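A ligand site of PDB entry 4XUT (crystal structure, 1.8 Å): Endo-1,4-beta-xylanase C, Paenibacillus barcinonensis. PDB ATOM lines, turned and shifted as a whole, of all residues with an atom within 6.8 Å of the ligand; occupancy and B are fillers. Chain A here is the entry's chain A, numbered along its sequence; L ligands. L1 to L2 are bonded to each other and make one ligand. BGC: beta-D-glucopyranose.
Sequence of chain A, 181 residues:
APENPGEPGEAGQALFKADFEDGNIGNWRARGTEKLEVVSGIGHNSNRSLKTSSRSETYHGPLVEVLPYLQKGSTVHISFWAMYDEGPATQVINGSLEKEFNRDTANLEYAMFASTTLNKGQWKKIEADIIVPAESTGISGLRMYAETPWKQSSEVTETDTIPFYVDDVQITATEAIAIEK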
ATOM      1  N   ARG A  29      21.107  -3.603  27.320  1.00  0.00           N
ATOM      2  CA  ARG A  29      22.290  -4.379  27.023  1.00  0.00           C
ATOM      3  C   ARG A  29      23.215  -3.652  26.067  1.00  0.00           C
ATOM      4  O   ARG A  29      22.804  -2.797  25.280  1.00  0.00           O
ATOM      5  CB  ARG A  29      21.959  -5.786  26.481  1.00  0.00           C
ATOM      6  CG  ARG A  29      21.256  -5.877  25.139  1.00  0.00           C
ATOM      7  CD  ARG A  29      21.351  -7.298  24.504  1.00  0.00           C
ATOM      8  NE  ARG A  29      20.698  -7.439  23.169  1.00  0.00           N
ATOM      9  CZ  ARG A  29      21.212  -7.041  21.985  1.00  0.00           C
ATOM     10  NH1 ARG A  29      22.408  -6.433  21.885  1.00  0.00           N
ATOM     11  NH2 ARG A  29      20.491  -7.227  20.849  1.00  0.00           N
ATOM     12  N   ALA A  30      24.485  -4.032  26.139  1.00  0.00           N
ATOM     13  CA  ALA A  30      25.473  -3.613  25.134  1.00  0.00           C
ATOM     14  C   ALA A  30      25.235  -4.315  23.812  1.00  0.00           C
ATOM     15  O   ALA A  30      24.628  -5.398  23.762  1.00  0.00           O
ATOM     16  CB  ALA A  30      26.883  -3.924  25.656  1.00  0.00           C
ATOM     17  N   ARG A  31      25.749  -3.716  22.728  1.00  0.00           N
ATOM     18  CA  ARG A  31      25.714  -4.342  21.412  1.00  0.00           C
ATOM     19  C   ARG A  31      26.994  -5.106  21.034  1.00  0.00           C
ATOM     20  O   ARG A  31      26.967  -5.998  20.210  1.00  0.00           O
ATOM     21  CB  ARG A  31      25.398  -3.280  20.357  1.00  0.00           C
ATOM     22  CG  ARG A  31      24.122  -2.518  20.714  1.00  0.00           C
ATOM     23  CD  ARG A  31      23.710  -1.594  19.597  1.00  0.00           C
ATOM     24  NE  ARG A  31      23.288  -2.408  18.462  1.00  0.00           N
ATOM     25  CZ  ARG A  31      23.738  -2.293  17.230  1.00  0.00           C
ATOM     26  NH1 ARG A  31      24.608  -1.351  16.887  1.00  0.00           N
ATOM     27  NH2 ARG A  31      23.267  -3.101  16.291  1.00  0.00           N
ATOM     28  N   GLY A  32      28.097  -4.736  21.667  1.00  0.00           N
ATOM     29  CA  GLY A  32      29.366  -5.447  21.481  1.00  0.00           C
ATOM     30  C   GLY A  32      30.102  -5.607  22.792  1.00  0.00           C
ATOM     31  O   GLY A  32      29.555  -6.132  23.741  1.00  0.00           O
ATOM     32  N   THR A  58      31.420   2.869  16.527  1.00  0.00           N
ATOM     33  CA  THR A  58      30.369   3.891  16.504  1.00  0.00           C
ATOM     34  C   THR A  58      29.017   3.302  16.870  1.00  0.00           C
ATOM     35  O   THR A  58      28.166   3.987  17.439  1.00  0.00           O
ATOM     36  CB  THR A  58      30.223   4.580  15.131  1.00  0.00           C
ATOM     37  OG1 THR A  58      29.937   3.599  14.113  1.00  0.00           O
ATOM     38  CG2 THR A  58      31.484   5.302  14.763  1.00  0.00           C
ATOM     39  N   TYR A  59      28.853   2.026  16.560  1.00  0.00           N
ATOM     40  CA  TYR A  59      27.595   1.326  16.782  1.00  0.00           C
ATOM     41  C   TYR A  59      27.473   0.694  18.173  1.00  0.00           C
ATOM     42  O   TYR A  59      26.485   0.081  18.478  1.00  0.00           O
ATOM     43  CB  TYR A  59      27.346   0.299  15.705  1.00  0.00           C
ATOM     44  CG  TYR A  59      28.455  -0.682  15.488  1.00  0.00           C
ATOM     45  CD1 TYR A  59      28.593  -1.814  16.282  1.00  0.00           C
ATOM     46  CD2 TYR A  59      29.355  -0.487  14.444  1.00  0.00           C
ATOM     47  CE1 TYR A  59      29.623  -2.741  16.053  1.00  0.00           C
ATOM     48  CE2 TYR A  59      30.392  -1.384  14.214  1.00  0.00           C
ATOM     49  CZ  TYR A  59      30.513  -2.506  14.999  1.00  0.00           C
ATOM     50  OH  TYR A  59      31.541  -3.369  14.723  1.00  0.00           O
ATOM     51  N   HIS A  60      28.478   0.893  19.020  1.00  0.00           N
ATOM     52  CA  HIS A  60      28.353   0.565  20.424  1.00  0.00           C
ATOM     53  C   HIS A  60      27.475   1.602  21.084  1.00  0.00           C
ATOM     54  O   HIS A  60      27.628   2.815  20.845  1.00  0.00           O
ATOM     55  CB  HIS A  60      29.720   0.534  21.097  1.00  0.00           C
ATOM     56  CG  HIS A  60      30.538  -0.659  20.723  1.00  0.00           C
ATOM     57  ND1 HIS A  60      31.846  -0.795  21.114  1.00  0.00           N
ATOM     58  CD2 HIS A  60      30.242  -1.760  20.004  1.00  0.00           C
ATOM     59  CE1 HIS A  60      32.326  -1.937  20.657  1.00  0.00           C
ATOM     60  NE2 HIS A  60      31.378  -2.552  19.983  1.00  0.00           N
ATOM     61  N   LEU A  63      21.146  -0.566  24.272  1.00  0.00           N
ATOM     62  CA  LEU A  63      20.071  -1.154  23.481  1.00  0.00           C
ATOM     63  C   LEU A  63      19.053  -1.804  24.397  1.00  0.00           C
ATOM     64  O   LEU A  63      19.394  -2.458  25.397  1.00  0.00           O
ATOM     65  CB  LEU A  63      20.669  -2.185  22.551  1.00  0.00           C
ATOM     66  CG  LEU A  63      19.695  -2.964  21.674  1.00  0.00           C
ATOM     67  CD1 LEU A  63      20.310  -3.263  20.313  1.00  0.00           C
ATOM     68  CD2 LEU A  63      19.235  -4.263  22.351  1.00  0.00           C
ATOM     69  N   SER A  96      18.344   4.726  16.997  1.00  0.00           N
ATOM     70  CA  SER A  96      18.245   3.730  15.945  1.00  0.00           C
ATOM     71  C   SER A  96      17.457   2.492  16.358  1.00  0.00           C
ATOM     72  O   SER A  96      17.204   2.268  17.543  1.00  0.00           O
ATOM     73  CB  SER A  96      19.612   3.281  15.447  1.00  0.00           C
ATOM     74  OG  SER A  96      20.331   4.356  14.864  1.00  0.00           O
ATOM     75  N   GLU A  98      17.196  -1.828  15.805  1.00  0.00           N
ATOM     76  CA  GLU A  98      17.714  -3.103  15.344  1.00  0.00           C
ATOM     77  C   GLU A  98      16.538  -4.011  15.206  1.00  0.00           C
ATOM     78  O   GLU A  98      15.775  -4.215  16.176  1.00  0.00           O
ATOM     79  CB  GLU A  98      18.718  -3.669  16.340  1.00  0.00           C
ATOM     80  CG  GLU A  98      19.267  -5.056  16.016  1.00  0.00           C
ATOM     81  CD  GLU A  98      20.258  -5.522  17.061  1.00  0.00           C
ATOM     82  OE1 GLU A  98      21.363  -4.969  17.119  1.00  0.00           O
ATOM     83  OE2 GLU A  98      19.910  -6.420  17.851  1.00  0.00           O
ATOM     84  N   LEU A 108      20.193  -9.408  10.673  1.00  0.00           N
ATOM     85  CA  LEU A 108      19.566  -8.243  11.319  1.00  0.00           C
ATOM     86  C   LEU A 108      19.594  -7.036  10.403  1.00  0.00           C
ATOM     87  O   LEU A 108      20.415  -6.984   9.460  1.00  0.00           O
ATOM     88  CB  LEU A 108      20.285  -7.907  12.615  1.00  0.00           C
ATOM     89  CG  LEU A 108      20.330  -9.016  13.665  1.00  0.00           C
ATOM     90  CD1 LEU A 108      21.063  -8.535  14.904  1.00  0.00           C
ATOM     91  CD2 LEU A 108      18.967  -9.523  14.053  1.00  0.00           C
ATOM     92  N   TYR A 110      19.171  -2.573  10.463  1.00  0.00           N
ATOM     93  CA  TYR A 110      19.419  -1.419  11.305  1.00  0.00           C
ATOM     94  C   TYR A 110      18.891  -0.199  10.617  1.00  0.00           C
ATOM     95  O   TYR A 110      19.059  -0.052   9.390  1.00  0.00           O
ATOM     96  CB  TYR A 110      20.908  -1.249  11.583  1.00  0.00           C
ATOM     97  CG  TYR A 110      21.557  -2.543  11.974  1.00  0.00           C
ATOM     98  CD1 TYR A 110      21.453  -3.023  13.277  1.00  0.00           C
ATOM     99  CD2 TYR A 110      22.274  -3.287  11.054  1.00  0.00           C
ATOM    100  CE1 TYR A 110      22.062  -4.229  13.626  1.00  0.00           C
ATOM    101  CE2 TYR A 110      22.840  -4.500  11.389  1.00  0.00           C
ATOM    102  CZ  TYR A 110      22.742  -4.964  12.687  1.00  0.00           C
ATOM    103  OH  TYR A 110      23.354  -6.163  13.004  1.00  0.00           O
ATOM    104  N   ALA A 111      18.228   0.681  11.360  1.00  0.00           N
ATOM    105  CA  ALA A 111      17.694   1.918  10.779  1.00  0.00           C
ATOM    106  C   ALA A 111      17.767   3.046  11.783  1.00  0.00           C
ATOM    107  O   ALA A 111      17.300   2.884  12.890  1.00  0.00           O
ATOM    108  CB  ALA A 111      16.254   1.709  10.380  1.00  0.00           C
ATOM    109  N   TYR A 145      18.116   1.589  20.184  1.00  0.00           N
ATOM    110  CA  TYR A 145      19.467   1.868  20.686  1.00  0.00           C
ATOM    111  C   TYR A 145      19.930   3.259  20.300  1.00  0.00           C
ATOM    112  O   TYR A 145      19.358   3.916  19.424  1.00  0.00           O
ATOM    113  CB  TYR A 145      20.464   0.803  20.292  1.00  0.00           C
ATOM    114  CG  TYR A 145      20.828   0.733  18.841  1.00  0.00           C
ATOM    115  CD1 TYR A 145      20.021   0.051  17.953  1.00  0.00           C
ATOM    116  CD2 TYR A 145      22.025   1.260  18.371  1.00  0.00           C
ATOM    117  CE1 TYR A 145      20.344  -0.023  16.619  1.00  0.00           C
ATOM    118  CE2 TYR A 145      22.370   1.153  17.043  1.00  0.00           C
ATOM    119  CZ  TYR A 145      21.516   0.515  16.172  1.00  0.00           C
ATOM    120  OH  TYR A 145      21.787   0.377  14.817  1.00  0.00           O
ATOM    121  N   GLU A 147      23.534   5.532  19.416  1.00  0.00           N
ATOM    122  CA  GLU A 147      24.862   5.311  18.846  1.00  0.00           C
ATOM    123  C   GLU A 147      25.365   6.635  18.282  1.00  0.00           C
ATOM    124  O   GLU A 147      24.690   7.646  18.349  1.00  0.00           O
ATOM    125  CB  GLU A 147      24.805   4.270  17.728  1.00  0.00           C
ATOM    126  CG  GLU A 147      23.965   4.701  16.541  1.00  0.00           C
ATOM    127  CD  GLU A 147      23.961   3.724  15.383  1.00  0.00           C
ATOM    128  OE1 GLU A 147      24.843   2.831  15.274  1.00  0.00           O
ATOM    129  OE2 GLU A 147      23.055   3.887  14.551  1.00  0.00           O
ATOM    130  N   THR A 148      26.599   6.659  17.790  1.00  0.00           N
ATOM    131  CA  THR A 148      27.108   7.808  17.052  1.00  0.00           C
ATOM    132  C   THR A 148      27.115   7.483  15.574  1.00  0.00           C
ATOM    133  O   THR A 148      27.034   6.291  15.223  1.00  0.00           O
ATOM    134  CB  THR A 148      28.511   8.256  17.560  1.00  0.00           C
ATOM    135  OG1 THR A 148      29.376   7.122  17.651  1.00  0.00           O
ATOM    136  CG2 THR A 148      28.393   8.885  18.916  1.00  0.00           C
ATOM    137  N   TRP A 150      27.799   6.369  11.859  1.00  0.00           N
ATOM    138  CA  TRP A 150      28.605   5.280  11.369  1.00  0.00           C
ATOM    139  C   TRP A 150      29.912   5.725  10.723  1.00  0.00           C
ATOM    140  O   TRP A 150      29.968   6.693   9.987  1.00  0.00           O
ATOM    141  CB  TRP A 150      27.819   4.393  10.417  1.00  0.00           C
ATOM    142  CG  TRP A 150      28.597   3.099  10.164  1.00  0.00           C
ATOM    143  CD1 TRP A 150      28.580   1.924  10.893  1.00  0.00           C
ATOM    144  CD2 TRP A 150      29.563   2.903   9.138  1.00  0.00           C
ATOM    145  NE1 TRP A 150      29.454   1.004  10.349  1.00  0.00           N
ATOM    146  CE2 TRP A 150      30.078   1.582   9.279  1.00  0.00           C
ATOM    147  CE3 TRP A 150      30.043   3.710   8.112  1.00  0.00           C
ATOM    148  CZ2 TRP A 150      31.040   1.071   8.399  1.00  0.00           C
ATOM    149  CZ3 TRP A 150      31.006   3.202   7.245  1.00  0.00           C
ATOM    150  CH2 TRP A 150      31.488   1.883   7.390  1.00  0.00           C
HETATM  151  C2  BGC L   1      28.311  -6.015  12.650  1.00  0.00           C
HETATM  152  C3  BGC L   1      28.092  -4.500  12.618  1.00  0.00           C
HETATM  153  C4  BGC L   1      26.835  -4.213  13.420  1.00  0.00           C
HETATM  154  C5  BGC L   1      27.048  -4.760  14.849  1.00  0.00           C
HETATM  155  C6  BGC L   1      25.849  -4.471  15.710  1.00  0.00           C
HETATM  156  C1  BGC L   1      28.582  -6.421  14.108  1.00  0.00           C
HETATM  157  O1  BGC L   1      29.026  -7.788  14.197  1.00  0.00           O
HETATM  158  O2  BGC L   1      29.326  -6.405  11.708  1.00  0.00           O
HETATM  159  O3  BGC L   1      27.953  -3.979  11.298  1.00  0.00           O
HETATM  160  O4  BGC L   1      26.647  -2.784  13.400  1.00  0.00           O
HETATM  161  O5  BGC L   1      27.384  -6.161  14.880  1.00  0.00           O
HETATM  162  O6  BGC L   1      26.037  -4.714  17.104  1.00  0.00           O
HETATM  163  C2  BGC L   2      25.392  -0.860  13.134  1.00  0.00           C
HETATM  164  C3  BGC L   2      24.591   0.160  12.350  1.00  0.00           C
HETATM  165  C4  BGC L   2      25.208   0.332  10.957  1.00  0.00           C
HETATM  166  C5  BGC L   2      25.432  -1.064  10.321  1.00  0.00           C
HETATM  167  C6  BGC L   2      26.002  -1.094   8.870  1.00  0.00           C
HETATM  168  C1  BGC L   2      25.733  -2.174  12.454  1.00  0.00           C
HETATM  169  O2  BGC L   2      24.693  -1.161  14.322  1.00  0.00           O
HETATM  170  O3  BGC L   2      24.531   1.415  13.078  1.00  0.00           O
HETATM  171  O4  BGC L   2      24.314   1.178  10.224  1.00  0.00           O
HETATM  172  O5  BGC L   2      26.277  -1.871  11.174  1.00  0.00           O
HETATM  173  O6  BGC L   2      27.297  -0.498   8.672  1.00  0.00           O
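The side-chain carboxylate (OE1) of Glu 147 sits at hydrogen-bond distance from an oxygen (O3) of BGC L2, 2.6 Å away.
O of Arg 31 lies close to O6 of BGC L1 (3.5 Å).
The guanidinium group (NH1) of Arg 31 lies within hydrogen-bond range of an oxygen (O2) of BGC L2 (2.6 Å).
The indole nitrogen (NE1) of Trp 150 lies within hydrogen-bond range of an oxygen (O6) of BGC L2 (3.1 Å).
O2 of BGC L2 is in hydrogen-bond range of OH of Tyr 145 (3.3 Å).
The guanidinium group (NH2) of Arg 31 is in salt-bridge range of the side-chain carboxylate (OE1) of Glu 98, at 2.8 Å.
The backbone carbonyl oxygen (O) of Tyr 59 is in hydrogen-bond range of the guanidinium group (NH1) of Arg 31.
The backbone carbonyl oxygen (O) of Tyr 145 lies within hydrogen-bond range of the backbone NH (N) of Ser 96 (2.8 Å).
The side-chain carboxylate of Glu 147 is in hydrogen-bond range of the side-chain hydroxyl of Ser 96.
Residues that only touch the ligand: Tyr 59 (3.3 Å) and Tyr 110 (3.9 Å).
Hydrophobic or aromatic side chains within 4 Å of the ligand: Tyr 59, Tyr 110 and Trp 150.
Six residues have an atom within 4 Å of the ligand: Arg 31, Tyr 59, Tyr 110, Tyr 145, Glu 147 and Trp 150.
The nearest printed residue that does not touch the ligand is Glu 98 (4.7 Å).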
